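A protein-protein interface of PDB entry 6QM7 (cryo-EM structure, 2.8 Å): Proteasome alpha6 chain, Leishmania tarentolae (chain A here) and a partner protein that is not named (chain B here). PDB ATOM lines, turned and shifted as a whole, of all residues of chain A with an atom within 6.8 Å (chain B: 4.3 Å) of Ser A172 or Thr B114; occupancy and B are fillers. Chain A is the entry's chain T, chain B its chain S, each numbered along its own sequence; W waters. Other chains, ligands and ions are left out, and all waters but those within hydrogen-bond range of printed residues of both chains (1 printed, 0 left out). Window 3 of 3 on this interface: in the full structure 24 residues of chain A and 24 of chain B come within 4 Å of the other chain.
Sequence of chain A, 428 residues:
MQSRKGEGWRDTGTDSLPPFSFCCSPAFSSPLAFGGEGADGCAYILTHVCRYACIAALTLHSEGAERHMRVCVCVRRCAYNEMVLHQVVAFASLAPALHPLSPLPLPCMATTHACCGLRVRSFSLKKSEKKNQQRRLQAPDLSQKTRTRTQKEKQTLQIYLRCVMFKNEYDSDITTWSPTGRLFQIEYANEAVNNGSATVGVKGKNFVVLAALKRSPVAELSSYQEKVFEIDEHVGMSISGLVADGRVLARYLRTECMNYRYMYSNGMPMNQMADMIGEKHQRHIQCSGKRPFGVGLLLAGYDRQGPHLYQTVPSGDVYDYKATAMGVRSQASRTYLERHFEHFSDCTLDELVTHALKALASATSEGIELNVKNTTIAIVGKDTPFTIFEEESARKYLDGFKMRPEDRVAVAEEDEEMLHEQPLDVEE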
ATOM      1  N   ASN A 168      19.061 -30.569 -32.200  1.00  0.00           N
ATOM      2  CA  ASN A 168      20.274 -29.704 -32.014  1.00  0.00           C
ATOM      3  C   ASN A 168      20.567 -29.601 -30.511  1.00  0.00           C
ATOM      4  O   ASN A 168      19.738 -29.003 -29.795  1.00  0.00           O
ATOM      5  CB  ASN A 168      20.083 -28.326 -32.660  1.00  0.00           C
ATOM      6  CG  ASN A 168      21.380 -27.594 -32.938  1.00  0.00           C
ATOM      7  OD1 ASN A 168      22.403 -27.853 -32.308  1.00  0.00           O
ATOM      8  ND2 ASN A 168      21.344 -26.667 -33.884  1.00  0.00           N
ATOM      9  N   GLU A 169      21.695 -30.158 -30.054  1.00  0.00           N
ATOM     10  CA  GLU A 169      22.059 -30.213 -28.605  1.00  0.00           C
ATOM     11  C   GLU A 169      22.833 -28.947 -28.201  1.00  0.00           C
ATOM     12  O   GLU A 169      23.161 -28.833 -27.001  1.00  0.00           O
ATOM     13  CB  GLU A 169      22.823 -31.491 -28.211  1.00  0.00           C
ATOM     14  CG  GLU A 169      23.740 -32.100 -29.269  1.00  0.00           C
ATOM     15  CD  GLU A 169      23.161 -33.268 -30.057  1.00  0.00           C
ATOM     16  OE1 GLU A 169      23.946 -34.162 -30.445  1.00  0.00           O
ATOM     17  OE2 GLU A 169      21.930 -33.291 -30.281  1.00  0.00           O
ATOM     18  N   TYR A 170      23.062 -28.011 -29.130  1.00  0.00           N
ATOM     19  CA  TYR A 170      23.972 -26.848 -28.958  1.00  0.00           C
ATOM     20  C   TYR A 170      23.221 -25.510 -28.983  1.00  0.00           C
ATOM     21  O   TYR A 170      23.902 -24.471 -28.831  1.00  0.00           O
ATOM     22  CB  TYR A 170      25.030 -26.875 -30.060  1.00  0.00           C
ATOM     23  CG  TYR A 170      25.878 -28.120 -30.057  1.00  0.00           C
ATOM     24  CD1 TYR A 170      26.786 -28.362 -29.037  1.00  0.00           C
ATOM     25  CD2 TYR A 170      25.763 -29.066 -31.065  1.00  0.00           C
ATOM     26  CE1 TYR A 170      27.566 -29.508 -29.021  1.00  0.00           C
ATOM     27  CE2 TYR A 170      26.534 -30.218 -31.063  1.00  0.00           C
ATOM     28  CZ  TYR A 170      27.440 -30.438 -30.039  1.00  0.00           C
ATOM     29  OH  TYR A 170      28.201 -31.569 -30.041  1.00  0.00           O
ATOM     30  N   ASP A 171      21.891 -25.510 -29.140  1.00  0.00           N
ATOM     31  CA  ASP A 171      21.090 -24.277 -29.385  1.00  0.00           C
ATOM     32  C   ASP A 171      20.376 -23.798 -28.108  1.00  0.00           C
ATOM     33  O   ASP A 171      19.683 -22.771 -28.187  1.00  0.00           O
ATOM     34  CB  ASP A 171      20.141 -24.497 -30.566  1.00  0.00           C
ATOM     35  CG  ASP A 171      18.848 -25.236 -30.255  1.00  0.00           C
ATOM     36  OD1 ASP A 171      18.810 -25.962 -29.239  1.00  0.00           O
ATOM     37  OD2 ASP A 171      17.887 -25.091 -31.046  1.00  0.00           O
ATOM     38  N   SER A 172      20.565 -24.480 -26.975  1.00  0.00           N
ATOM     39  CA  SER A 172      19.800 -24.269 -25.718  1.00  0.00           C
ATOM     40  C   SER A 172      20.399 -23.092 -24.940  1.00  0.00           C
ATOM     41  O   SER A 172      19.636 -22.180 -24.589  1.00  0.00           O
ATOM     42  CB  SER A 172      19.759 -25.525 -24.860  1.00  0.00           C
ATOM     43  OG  SER A 172      20.011 -26.696 -25.624  1.00  0.00           O
ATOM     44  N   ASP A 173      21.707 -23.129 -24.667  1.00  0.00           N
ATOM     45  CA  ASP A 173      22.421 -22.143 -23.809  1.00  0.00           C
ATOM     46  C   ASP A 173      23.200 -21.161 -24.698  1.00  0.00           C
ATOM     47  O   ASP A 173      23.632 -21.537 -25.809  1.00  0.00           O
ATOM     48  CB  ASP A 173      23.318 -22.855 -22.783  1.00  0.00           C
ATOM     49  CG  ASP A 173      23.453 -22.162 -21.421  1.00  0.00           C
ATOM     50  OD1 ASP A 173      23.534 -20.907 -21.384  1.00  0.00           O
ATOM     51  OD2 ASP A 173      23.484 -22.883 -20.389  1.00  0.00           O
ATOM     52  N   ILE A 174      23.346 -19.932 -24.217  1.00  0.00           N
ATOM     53  CA  ILE A 174      24.192 -18.870 -24.835  1.00  0.00           C
ATOM     54  C   ILE A 174      25.676 -19.244 -24.729  1.00  0.00           C
ATOM     55  O   ILE A 174      26.418 -18.899 -25.656  1.00  0.00           O
ATOM     56  CB  ILE A 174      23.898 -17.491 -24.200  1.00  0.00           C
ATOM     57  CG1 ILE A 174      24.552 -16.342 -24.976  1.00  0.00           C
ATOM     58  CG2 ILE A 174      24.295 -17.444 -22.730  1.00  0.00           C
ATOM     59  CD1 ILE A 174      24.136 -16.234 -26.424  1.00  0.00           C
ATOM     60  N   THR A 175      26.085 -19.935 -23.666  1.00  0.00           N
ATOM     61  CA  THR A 175      27.500 -20.301 -23.372  1.00  0.00           C
ATOM     62  C   THR A 175      27.968 -21.498 -24.206  1.00  0.00           C
ATOM     63  O   THR A 175      29.128 -21.914 -24.019  1.00  0.00           O
ATOM     64  CB  THR A 175      27.707 -20.730 -21.913  1.00  0.00           C
ATOM     65  OG1 THR A 175      27.021 -21.959 -21.673  1.00  0.00           O
ATOM     66  CG2 THR A 175      27.238 -19.689 -20.925  1.00  0.00           C
ATOM     67  N   THR A 176      27.120 -22.070 -25.059  1.00  0.00           N
ATOM     68  CA  THR A 176      27.500 -23.254 -25.851  1.00  0.00           C
ATOM     69  C   THR A 176      27.826 -22.846 -27.282  1.00  0.00           C
ATOM     70  O   THR A 176      26.904 -22.482 -28.021  1.00  0.00           O
ATOM     71  CB  THR A 176      26.418 -24.323 -25.790  1.00  0.00           C
ATOM     72  OG1 THR A 176      26.164 -24.552 -24.404  1.00  0.00           O
ATOM     73  CG2 THR A 176      26.857 -25.593 -26.483  1.00  0.00           C
ATOM     74  N   PHE A 184      24.238 -20.329 -31.436  1.00  0.00           N
ATOM     75  CA  PHE A 184      22.862 -20.427 -31.973  1.00  0.00           C
ATOM     76  C   PHE A 184      21.926 -19.473 -31.235  1.00  0.00           C
ATOM     77  O   PHE A 184      21.104 -18.840 -31.897  1.00  0.00           O
ATOM     78  CB  PHE A 184      22.363 -21.864 -31.905  1.00  0.00           C
ATOM     79  CG  PHE A 184      22.798 -22.711 -33.068  1.00  0.00           C
ATOM     80  CD1 PHE A 184      22.201 -22.561 -34.307  1.00  0.00           C
ATOM     81  CD2 PHE A 184      23.788 -23.667 -32.922  1.00  0.00           C
ATOM     82  CE1 PHE A 184      22.583 -23.355 -35.377  1.00  0.00           C
ATOM     83  CE2 PHE A 184      24.165 -24.464 -33.992  1.00  0.00           C
ATOM     84  CZ  PHE A 184      23.563 -24.307 -35.217  1.00  0.00           C
ATOM     85  N   GLN A 185      22.043 -19.343 -29.920  1.00  0.00           N
ATOM     86  CA  GLN A 185      21.154 -18.428 -29.159  1.00  0.00           C
ATOM     87  C   GLN A 185      21.275 -17.003 -29.707  1.00  0.00           C
ATOM     88  O   GLN A 185      20.276 -16.265 -29.613  1.00  0.00           O
ATOM     89  CB  GLN A 185      21.419 -18.478 -27.654  1.00  0.00           C
ATOM     90  CG  GLN A 185      20.673 -19.612 -26.959  1.00  0.00           C
ATOM     91  CD  GLN A 185      19.177 -19.453 -27.048  1.00  0.00           C
ATOM     92  OE1 GLN A 185      18.603 -18.570 -26.423  1.00  0.00           O
ATOM     93  NE2 GLN A 185      18.544 -20.298 -27.846  1.00  0.00           N
ATOM     94  N   TYR A 188      19.422 -16.927 -33.145  1.00  0.00           N
ATOM     95  CA  TYR A 188      17.972 -16.982 -32.839  1.00  0.00           C
ATOM     96  C   TYR A 188      17.501 -15.623 -32.345  1.00  0.00           C
ATOM     97  O   TYR A 188      16.415 -15.205 -32.753  1.00  0.00           O
ATOM     98  CB  TYR A 188      17.663 -18.053 -31.794  1.00  0.00           C
ATOM     99  CG  TYR A 188      17.885 -19.482 -32.230  1.00  0.00           C
ATOM    100  CD1 TYR A 188      18.150 -19.827 -33.546  1.00  0.00           C
ATOM    101  CD2 TYR A 188      17.776 -20.504 -31.305  1.00  0.00           C
ATOM    102  CE1 TYR A 188      18.335 -21.148 -33.919  1.00  0.00           C
ATOM    103  CE2 TYR A 188      17.938 -21.831 -31.667  1.00  0.00           C
ATOM    104  CZ  TYR A 188      18.230 -22.158 -32.977  1.00  0.00           C
ATOM    105  OH  TYR A 188      18.402 -23.464 -33.329  1.00  0.00           O
ATOM    106  N   ARG A 291      21.030 -13.319 -21.292  1.00  0.00           N
ATOM    107  CA  ARG A 291      20.663 -13.723 -22.677  1.00  0.00           C
ATOM    108  C   ARG A 291      20.859 -12.544 -23.617  1.00  0.00           C
ATOM    109  O   ARG A 291      20.756 -11.395 -23.198  1.00  0.00           O
ATOM    110  CB  ARG A 291      19.205 -14.173 -22.773  1.00  0.00           C
ATOM    111  CG  ARG A 291      18.185 -13.042 -22.756  1.00  0.00           C
ATOM    112  CD  ARG A 291      16.764 -13.502 -22.989  1.00  0.00           C
ATOM    113  NE  ARG A 291      15.817 -12.501 -22.542  1.00  0.00           N
ATOM    114  CZ  ARG A 291      15.565 -11.352 -23.166  1.00  0.00           C
ATOM    115  NH1 ARG A 291      16.165 -11.038 -24.307  1.00  0.00           N
ATOM    116  NH2 ARG A 291      14.666 -10.528 -22.655  1.00  0.00           N
ATOM    117  N   GLY B 111      16.774 -23.500 -20.398  1.00  0.00           N
ATOM    118  CA  GLY B 111      16.801 -22.404 -19.414  1.00  0.00           C
ATOM    119  C   GLY B 111      15.636 -21.446 -19.611  1.00  0.00           C
ATOM    120  O   GLY B 111      14.999 -21.464 -20.678  1.00  0.00           O
ATOM    121  N   VAL B 112      15.377 -20.625 -18.600  1.00  0.00           N
ATOM    122  CA  VAL B 112      14.300 -19.590 -18.577  1.00  0.00           C
ATOM    123  C   VAL B 112      14.569 -18.522 -19.654  1.00  0.00           C
ATOM    124  O   VAL B 112      13.588 -18.045 -20.271  1.00  0.00           O
ATOM    125  CB  VAL B 112      14.198 -18.995 -17.155  1.00  0.00           C
ATOM    126  CG1 VAL B 112      13.656 -17.575 -17.133  1.00  0.00           C
ATOM    127  CG2 VAL B 112      13.381 -19.902 -16.244  1.00  0.00           C
ATOM    128  N   ASN B 113      15.843 -18.177 -19.880  1.00  0.00           N
ATOM    129  CA  ASN B 113      16.293 -16.997 -20.669  1.00  0.00           C
ATOM    130  C   ASN B 113      16.669 -17.444 -22.085  1.00  0.00           C
ATOM    131  O   ASN B 113      17.548 -16.829 -22.694  1.00  0.00           O
ATOM    132  CB  ASN B 113      17.452 -16.287 -19.951  1.00  0.00           C
ATOM    133  CG  ASN B 113      17.038 -15.093 -19.112  1.00  0.00           C
ATOM    134  OD1 ASN B 113      15.870 -14.699 -19.080  1.00  0.00           O
ATOM    135  ND2 ASN B 113      18.004 -14.498 -18.431  1.00  0.00           N
ATOM    136  N   THR B 114      15.997 -18.458 -22.613  1.00  0.00           N
ATOM    137  CA  THR B 114      16.370 -19.150 -23.871  1.00  0.00           C
ATOM    138  C   THR B 114      15.405 -18.753 -24.984  1.00  0.00           C
ATOM    139  O   THR B 114      14.186 -18.939 -24.791  1.00  0.00           O
ATOM    140  CB  THR B 114      16.331 -20.665 -23.680  1.00  0.00           C
ATOM    141  OG1 THR B 114      17.404 -20.996 -22.804  1.00  0.00           O
ATOM    142  CG2 THR B 114      16.467 -21.433 -24.974  1.00  0.00           C
ATOM    143  N   PHE B 115      15.948 -18.269 -26.101  1.00  0.00           N
ATOM    144  CA  PHE B 115      15.222 -18.006 -27.366  1.00  0.00           C
ATOM    145  C   PHE B 115      14.899 -19.321 -28.064  1.00  0.00           C
ATOM    146  O   PHE B 115      15.686 -20.283 -27.947  1.00  0.00           O
ATOM    147  CB  PHE B 115      16.065 -17.176 -28.328  1.00  0.00           C
ATOM    148  CG  PHE B 115      16.183 -15.733 -27.938  1.00  0.00           C
ATOM    149  CD1 PHE B 115      15.296 -14.799 -28.431  1.00  0.00           C
ATOM    150  CD2 PHE B 115      17.187 -15.315 -27.088  1.00  0.00           C
ATOM    151  CE1 PHE B 115      15.398 -13.467 -28.071  1.00  0.00           C
ATOM    152  CE2 PHE B 115      17.288 -13.986 -26.714  1.00  0.00           C
ATOM    153  CZ  PHE B 115      16.386 -13.064 -27.205  1.00  0.00           C
ATOM    154  N   SER B 116      13.770 -19.324 -28.777  1.00  0.00           N
ATOM    155  CA  SER B 116      13.360 -20.355 -29.761  1.00  0.00           C
ATOM    156  C   SER B 116      14.038 -20.049 -31.086  1.00  0.00           C
ATOM    157  O   SER B 116      14.511 -18.933 -31.273  1.00  0.00           O
ATOM    158  CB  SER B 116      11.849 -20.399 -29.916  1.00  0.00           C
ATOM    159  OG  SER B 116      11.351 -19.275 -30.634  1.00  0.00           O
ATOM    160  N   ILE B 121      11.347 -15.698 -26.898  1.00  0.00           N
ATOM    161  CA  ILE B 121      11.722 -16.303 -25.591  1.00  0.00           C
ATOM    162  C   ILE B 121      10.607 -17.274 -25.211  1.00  0.00           C
ATOM    163  O   ILE B 121       9.462 -16.842 -25.174  1.00  0.00           O
ATOM    164  CB  ILE B 121      11.962 -15.214 -24.530  1.00  0.00           C
ATOM    165  CG1 ILE B 121      13.139 -14.313 -24.906  1.00  0.00           C
ATOM    166  CG2 ILE B 121      12.160 -15.826 -23.152  1.00  0.00           C
ATOM    167  CD1 ILE B 121      13.005 -12.921 -24.355  1.00  0.00           C
ATOM    168  N   PHE B 122      10.937 -18.539 -24.969  1.00  0.00           N
ATOM    169  CA  PHE B 122       9.962 -19.615 -24.658  1.00  0.00           C
ATOM    170  C   PHE B 122       9.093 -19.242 -23.452  1.00  0.00           C
ATOM    171  O   PHE B 122       7.869 -19.192 -23.617  1.00  0.00           O
ATOM    172  CB  PHE B 122      10.675 -20.937 -24.401  1.00  0.00           C
ATOM    173  CG  PHE B 122      11.130 -21.636 -25.651  1.00  0.00           C
ATOM    174  CD1 PHE B 122      10.199 -22.181 -26.525  1.00  0.00           C
ATOM    175  CD2 PHE B 122      12.478 -21.767 -25.947  1.00  0.00           C
ATOM    176  CE1 PHE B 122      10.603 -22.842 -27.674  1.00  0.00           C
ATOM    177  CE2 PHE B 122      12.884 -22.427 -27.095  1.00  0.00           C
ATOM    178  CZ  PHE B 122      11.947 -22.962 -27.957  1.00  0.00           C
HETATM  179  O   HOH W   1      13.892 -13.116 -20.695  1.00  0.00           O
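NE2 of Gln A185 lies within hydrogen-bond range of O of Asp A171 (2.7 Å).
O of Gly B111 is in hydrogen-bond range of OG1 of Thr B114, at 3.2 Å.
The side-chain carboxylate of Asp A171 sits at hydrogen-bond distance from the side-chain hydroxyl of Tyr A188.
O of Thr B114 lies within hydrogen-bond range of N of Phe B122 (3.3 Å).
Of the 13 printed residues of chain A, 4 touch a printed residue of chain B.
Printed residues of chain A that touch a printed residue of chain B: Ser A172, Gln A185, Tyr A188 and Arg A291.
Ser A172 touches just one residue of chain B: Thr B114.
Ile A174 touches none of the printed residues of chain B.
Of the printed residues of chain B, Arg A291 touches Asn B113, Phe B115 and Ile B121.
Printed residues of chain A within 4 Å of Asn B113: Arg A291.
Of the printed residues of chain A, Thr B114 touches Ser A172 (3.1 Å) and Gln A185 (3.4 Å).
The nearest printed residue of chain B that does not touch Ser A172 is Gly B111 (5.2 Å).
The nearest residue of chain A that does not touch Thr B114 is Asp A171 (4.7 Å).
The nearest printed residue of chain A that does not touch Ser B116 is Gln A185 (5.0 Å).
Among the printed residues, pairs that only touch across the chains: Arg A291 with Asn B113 (3.1 Å), Arg A291 with Ile B121 (3.2 Å), Tyr A188 with Ser B116 (3.3 Å), Gln A185 with Thr B114 (3.4 Å), Arg A291 with Phe B115 (3.5 Å) and Tyr A188 with Phe B115 (3.9 Å).
The backbone NH (N) of Phe B115 sits at hydrogen-bond distance from the side-chain amide oxygen (OE1) of Gln A185, 2.7 Å away.
OG1 of Thr B114 lies within hydrogen-bond range of O of Ser A172.
Water W1 bridges the guanidinium group (NE) of Arg A291 and the side-chain amide oxygen (OD1) of Asn B113.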
